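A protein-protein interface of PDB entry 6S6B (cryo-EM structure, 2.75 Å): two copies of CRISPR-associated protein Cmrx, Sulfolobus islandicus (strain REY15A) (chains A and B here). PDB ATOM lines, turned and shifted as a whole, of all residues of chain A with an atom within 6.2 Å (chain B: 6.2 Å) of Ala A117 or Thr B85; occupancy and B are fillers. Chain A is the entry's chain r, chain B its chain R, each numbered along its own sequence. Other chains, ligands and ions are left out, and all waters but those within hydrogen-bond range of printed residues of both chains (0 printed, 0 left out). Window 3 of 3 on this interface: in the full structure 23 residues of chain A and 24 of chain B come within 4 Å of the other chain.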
ATOM      1  N   SER A 114      18.824  -2.148  -1.171  1.00  0.00           N
ATOM      2  CA  SER A 114      17.978  -1.144  -0.556  1.00  0.00           C
ATOM      3  C   SER A 114      16.893  -1.844   0.258  1.00  0.00           C
ATOM      4  O   SER A 114      16.468  -2.951  -0.086  1.00  0.00           O
ATOM      5  CB  SER A 114      17.346  -0.248  -1.618  1.00  0.00           C
ATOM      6  OG  SER A 114      18.331   0.468  -2.343  1.00  0.00           O
ATOM      7  N   PRO A 115      16.456  -1.243   1.362  1.00  0.00           N
ATOM      8  CA  PRO A 115      15.382  -1.856   2.153  1.00  0.00           C
ATOM      9  C   PRO A 115      14.175  -2.186   1.294  1.00  0.00           C
ATOM     10  O   PRO A 115      13.535  -1.289   0.736  1.00  0.00           O
ATOM     11  CB  PRO A 115      15.060  -0.782   3.197  1.00  0.00           C
ATOM     12  CG  PRO A 115      16.333  -0.028   3.347  1.00  0.00           C
ATOM     13  CD  PRO A 115      16.985  -0.023   1.993  1.00  0.00           C
ATOM     14  N   ASP A 116      13.863  -3.476   1.178  1.00  0.00           N
ATOM     15  CA  ASP A 116      12.812  -3.942   0.275  1.00  0.00           C
ATOM     16  C   ASP A 116      11.460  -3.558   0.865  1.00  0.00           C
ATOM     17  O   ASP A 116      10.773  -4.347   1.519  1.00  0.00           O
ATOM     18  CB  ASP A 116      12.917  -5.446   0.048  1.00  0.00           C
ATOM     19  CG  ASP A 116      12.174  -5.904  -1.200  1.00  0.00           C
ATOM     20  OD1 ASP A 116      11.213  -5.217  -1.616  1.00  0.00           O
ATOM     21  OD2 ASP A 116      12.552  -6.951  -1.766  1.00  0.00           O
ATOM     22  N   ALA A 117      11.071  -2.311   0.614  1.00  0.00           N
ATOM     23  CA  ALA A 117       9.763  -1.819   1.016  1.00  0.00           C
ATOM     24  C   ALA A 117       8.728  -2.362   0.037  1.00  0.00           C
ATOM     25  O   ALA A 117       8.995  -3.296  -0.724  1.00  0.00           O
ATOM     26  CB  ALA A 117       9.763  -0.296   1.096  1.00  0.00           C
ATOM     27  N   ARG A 118       7.522  -1.795   0.064  1.00  0.00           N
ATOM     28  CA  ARG A 118       6.339  -2.267  -0.650  1.00  0.00           C
ATOM     29  C   ARG A 118       5.831  -3.578  -0.074  1.00  0.00           C
ATOM     30  O   ARG A 118       4.763  -4.046  -0.477  1.00  0.00           O
ATOM     31  CB  ARG A 118       6.574  -2.456  -2.159  1.00  0.00           C
ATOM     32  CG  ARG A 118       6.630  -1.183  -2.991  1.00  0.00           C
ATOM     33  CD  ARG A 118       7.938  -0.427  -2.795  1.00  0.00           C
ATOM     34  NE  ARG A 118       9.097  -1.310  -2.842  1.00  0.00           N
ATOM     35  CZ  ARG A 118      10.314  -0.962  -2.435  1.00  0.00           C
ATOM     36  NH1 ARG A 118      10.535   0.259  -1.975  1.00  0.00           N
ATOM     37  NH2 ARG A 118      11.313  -1.830  -2.503  1.00  0.00           N
ATOM     38  N   ASN A 119       6.554  -4.175   0.867  1.00  0.00           N
ATOM     39  CA  ASN A 119       6.158  -5.413   1.514  1.00  0.00           C
ATOM     40  C   ASN A 119       6.673  -5.384   2.940  1.00  0.00           C
ATOM     41  O   ASN A 119       7.775  -4.894   3.204  1.00  0.00           O
ATOM     42  CB  ASN A 119       6.721  -6.651   0.798  1.00  0.00           C
ATOM     43  CG  ASN A 119       6.310  -6.727  -0.657  1.00  0.00           C
ATOM     44  OD1 ASN A 119       5.125  -6.700  -0.982  1.00  0.00           O
ATOM     45  ND2 ASN A 119       7.295  -6.828  -1.543  1.00  0.00           N
ATOM     46  N   SER A 120       5.871  -5.902   3.861  1.00  0.00           N
ATOM     47  CA  SER A 120       6.389  -6.215   5.181  1.00  0.00           C
ATOM     48  C   SER A 120       7.304  -7.422   5.062  1.00  0.00           C
ATOM     49  O   SER A 120       7.009  -8.366   4.325  1.00  0.00           O
ATOM     50  CB  SER A 120       5.253  -6.484   6.163  1.00  0.00           C
ATOM     51  OG  SER A 120       4.495  -5.307   6.363  1.00  0.00           O
ATOM     52  N   MET A 121       8.435  -7.371   5.768  1.00  0.00           N
ATOM     53  CA  MET A 121       9.512  -8.327   5.540  1.00  0.00           C
ATOM     54  C   MET A 121       9.004  -9.765   5.574  1.00  0.00           C
ATOM     55  O   MET A 121       9.026 -10.466   4.557  1.00  0.00           O
ATOM     56  CB  MET A 121      10.617  -8.111   6.572  1.00  0.00           C
ATOM     57  CG  MET A 121      11.336  -6.782   6.428  1.00  0.00           C
ATOM     58  SD  MET A 121      12.545  -6.772   5.093  1.00  0.00           S
ATOM     59  CE  MET A 121      12.875  -5.018   4.969  1.00  0.00           C
ATOM     60  N   PRO B  75       9.317  10.963   7.519  1.00  0.00           N
ATOM     61  CA  PRO B  75      10.526  11.747   7.814  1.00  0.00           C
ATOM     62  C   PRO B  75      10.561  13.093   7.103  1.00  0.00           C
ATOM     63  O   PRO B  75      10.771  13.171   5.888  1.00  0.00           O
ATOM     64  CB  PRO B  75      11.658  10.822   7.344  1.00  0.00           C
ATOM     65  CG  PRO B  75      11.054  10.013   6.266  1.00  0.00           C
ATOM     66  CD  PRO B  75       9.599   9.836   6.611  1.00  0.00           C
ATOM     67  N   SER B  80      13.964  12.161   0.754  1.00  0.00           N
ATOM     68  CA  SER B  80      14.061  10.807   1.295  1.00  0.00           C
ATOM     69  C   SER B  80      15.381  10.154   0.901  1.00  0.00           C
ATOM     70  O   SER B  80      15.428   9.044   0.376  1.00  0.00           O
ATOM     71  CB  SER B  80      12.872   9.973   0.834  1.00  0.00           C
ATOM     72  OG  SER B  80      11.672  10.430   1.435  1.00  0.00           O
ATOM     73  N   PHE B  83      16.293   7.975   5.179  1.00  0.00           N
ATOM     74  CA  PHE B  83      15.617   7.055   6.077  1.00  0.00           C
ATOM     75  C   PHE B  83      15.344   5.709   5.417  1.00  0.00           C
ATOM     76  O   PHE B  83      15.219   5.602   4.195  1.00  0.00           O
ATOM     77  CB  PHE B  83      14.324   7.684   6.595  1.00  0.00           C
ATOM     78  CG  PHE B  83      14.561   8.856   7.500  1.00  0.00           C
ATOM     79  CD1 PHE B  83      14.990  10.068   6.987  1.00  0.00           C
ATOM     80  CD2 PHE B  83      14.389   8.739   8.865  1.00  0.00           C
ATOM     81  CE1 PHE B  83      15.227  11.141   7.813  1.00  0.00           C
ATOM     82  CE2 PHE B  83      14.625   9.814   9.699  1.00  0.00           C
ATOM     83  CZ  PHE B  83      15.043  11.016   9.169  1.00  0.00           C
ATOM     84  N   LEU B  84      15.258   4.675   6.258  1.00  0.00           N
ATOM     85  CA  LEU B  84      15.222   3.304   5.764  1.00  0.00           C
ATOM     86  C   LEU B  84      13.985   3.033   4.921  1.00  0.00           C
ATOM     87  O   LEU B  84      14.073   2.368   3.882  1.00  0.00           O
ATOM     88  CB  LEU B  84      15.285   2.326   6.934  1.00  0.00           C
ATOM     89  CG  LEU B  84      16.688   2.003   7.431  1.00  0.00           C
ATOM     90  CD1 LEU B  84      16.638   0.883   8.448  1.00  0.00           C
ATOM     91  CD2 LEU B  84      17.580   1.629   6.263  1.00  0.00           C
ATOM     92  N   THR B  85      12.823   3.527   5.356  1.00  0.00           N
ATOM     93  CA  THR B  85      11.545   3.218   4.716  1.00  0.00           C
ATOM     94  C   THR B  85      11.320   1.703   4.695  1.00  0.00           C
ATOM     95  O   THR B  85      11.326   1.045   3.653  1.00  0.00           O
ATOM     96  CB  THR B  85      11.468   3.816   3.305  1.00  0.00           C
ATOM     97  OG1 THR B  85      11.923   5.175   3.334  1.00  0.00           O
ATOM     98  CG2 THR B  85      10.042   3.772   2.777  1.00  0.00           C
ATOM     99  N   LEU B  86      11.161   1.161   5.898  1.00  0.00           N
ATOM    100  CA  LEU B  86      11.074  -0.276   6.106  1.00  0.00           C
ATOM    101  C   LEU B  86       9.669  -0.663   6.541  1.00  0.00           C
ATOM    102  O   LEU B  86       9.026   0.053   7.314  1.00  0.00           O
ATOM    103  CB  LEU B  86      12.089  -0.723   7.157  1.00  0.00           C
ATOM    104  CG  LEU B  86      12.556  -2.176   7.105  1.00  0.00           C
ATOM    105  CD1 LEU B  86      13.956  -2.290   7.687  1.00  0.00           C
ATOM    106  CD2 LEU B  86      11.601  -3.110   7.825  1.00  0.00           C
ATOM    107  N   LYS B  87       9.197  -1.801   6.036  1.00  0.00           N
ATOM    108  CA  LYS B  87       7.918  -2.378   6.422  1.00  0.00           C
ATOM    109  C   LYS B  87       8.161  -3.744   7.044  1.00  0.00           C
ATOM    110  O   LYS B  87       8.949  -4.538   6.521  1.00  0.00           O
ATOM    111  CB  LYS B  87       6.984  -2.523   5.217  1.00  0.00           C
ATOM    112  CG  LYS B  87       6.616  -1.213   4.546  1.00  0.00           C
ATOM    113  CD  LYS B  87       5.875  -1.437   3.237  1.00  0.00           C
ATOM    114  CE  LYS B  87       4.454  -1.916   3.476  1.00  0.00           C
ATOM    115  NZ  LYS B  87       3.692  -2.069   2.203  1.00  0.00           N
ATOM    116  N   LYS B 107       4.917  -0.131   8.802  1.00  0.00           N
ATOM    117  CA  LYS B 107       5.893   0.544   7.961  1.00  0.00           C
ATOM    118  C   LYS B 107       6.608   1.602   8.785  1.00  0.00           C
ATOM    119  O   LYS B 107       5.967   2.507   9.330  1.00  0.00           O
ATOM    120  CB  LYS B 107       5.208   1.174   6.754  1.00  0.00           C
ATOM    121  CG  LYS B 107       6.104   2.088   5.947  1.00  0.00           C
ATOM    122  CD  LYS B 107       5.615   2.203   4.522  1.00  0.00           C
ATOM    123  CE  LYS B 107       6.517   3.101   3.711  1.00  0.00           C
ATOM    124  NZ  LYS B 107       5.913   4.445   3.507  1.00  0.00           N
ATOM    125  N   ILE B 108       7.930   1.495   8.882  1.00  0.00           N
ATOM    126  CA  ILE B 108       8.698   2.350   9.774  1.00  0.00           C
ATOM    127  C   ILE B 108       9.835   3.007   9.008  1.00  0.00           C
ATOM    128  O   ILE B 108      10.334   2.474   8.011  1.00  0.00           O
ATOM    129  CB  ILE B 108       9.247   1.571  10.985  1.00  0.00           C
ATOM    130  CG1 ILE B 108      10.122   0.411  10.525  1.00  0.00           C
ATOM    131  CG2 ILE B 108       8.108   1.048  11.831  1.00  0.00           C
ATOM    132  CD1 ILE B 108      10.712  -0.381  11.662  1.00  0.00           C
ATOM    133  N   TYR B 109      10.241   4.179   9.486  1.00  0.00           N
ATOM    134  CA  TYR B 109      11.351   4.933   8.926  1.00  0.00           C
ATOM    135  C   TYR B 109      12.414   5.101   9.998  1.00  0.00           C
ATOM    136  O   TYR B 109      12.096   5.431  11.145  1.00  0.00           O
ATOM    137  CB  TYR B 109      10.896   6.300   8.413  1.00  0.00           C
ATOM    138  CG  TYR B 109       9.953   6.243   7.234  1.00  0.00           C
ATOM    139  CD1 TYR B 109       8.625   5.873   7.395  1.00  0.00           C
ATOM    140  CD2 TYR B 109      10.392   6.561   5.959  1.00  0.00           C
ATOM    141  CE1 TYR B 109       7.763   5.823   6.322  1.00  0.00           C
ATOM    142  CE2 TYR B 109       9.538   6.519   4.881  1.00  0.00           C
ATOM    143  CZ  TYR B 109       8.226   6.146   5.067  1.00  0.00           C
ATOM    144  OH  TYR B 109       7.374   6.100   3.990  1.00  0.00           O
ATOM    145  N   ILE B 110      13.667   4.877   9.625  1.00  0.00           N
ATOM    146  CA  ILE B 110      14.771   4.870  10.578  1.00  0.00           C
ATOM    147  C   ILE B 110      15.846   5.831  10.088  1.00  0.00           C
ATOM    148  O   ILE B 110      16.162   5.845   8.892  1.00  0.00           O
ATOM    149  CB  ILE B 110      15.330   3.449  10.763  1.00  0.00           C
ATOM    150  CG1 ILE B 110      14.250   2.512  11.305  1.00  0.00           C
ATOM    151  CG2 ILE B 110      16.531   3.449  11.686  1.00  0.00           C
ATOM    152  CD1 ILE B 110      13.572   1.680  10.241  1.00  0.00           C
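O of Lys B87 is in hydrogen-bond range of N of Met A121 (3.0 Å).
The side-chain amino group (NZ) of Lys B87 lies close to the backbone carbonyl oxygen (O) of Arg A118 (3.5 Å).
The backbone NH (N) of Leu B86 lies within hydrogen-bond range of the backbone carbonyl oxygen (O) of Ile B108, at 2.6 Å.
The side-chain hydroxyl of Thr B85 lies within hydrogen-bond range of the backbone carbonyl oxygen of Phe B83 (3.4 Å).
The guanidinium group (NH2) of Arg A118 is in salt-bridge range of the side-chain carboxylate (OD1) of Asp A116 (3.5 Å).
N of Leu B84 is in hydrogen-bond range of O of Ile B110, at 3.0 Å.
CG of Pro A115 touches O of Leu B84, at 3.3 Å.
Ala A117 touches Thr B85.
Asn A119 touches Lys B87.
Ser A120 touches Lys B87 (CA to O, 3.3 Å).
CG of Leu B86 touches CE of Met A121, at 3.6 Å.
Printed residues of chain B within 4 Å of Pro A115: Leu B84.
Ala A117 touches just one residue of chain B: Thr B85 (3.3 Å).
Ser B80 touches none of the printed residues of chain A.
Of the printed residues of chain A, Leu B84 touches Pro A115 (3.3 Å).
Of chain A, only Ala A117 comes within 4 Å of Thr B85.
Ile B110 touches none of the printed residues of chain A.
The nearest residue of chain B that does not touch Ala A117 is Lys B87 (4.4 Å).
The nearest residue of chain A that does not touch Thr B85 is Pro A115 (4.2 Å).
The nearest printed residue of chain B that does not touch Asn A119 is Leu B86 (5.7 Å).
Hydrophobic or aromatic side chains of chain A within 4 Å of the printed part of chain B: Pro A115, Ala A117 and Met A121.
Of the 11 printed residues of chain B, 4 touch a printed residue of chain A.
Hydrophobic or aromatic side chains of chain B within 4 Å of the printed part of chain A: Leu B84 and Leu B86.
Among the printed residues, 7 pairs touch across the chains.
Among the printed residues, no Asp or Glu carboxylate lies within 4 Å of a Lys or Arg side-chain nitrogen of the other chain.
No position is printed for both chains.
Of the 7 pairs that touch across the chains among the printed residues, none has its exchanged pair printed and touching as well.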
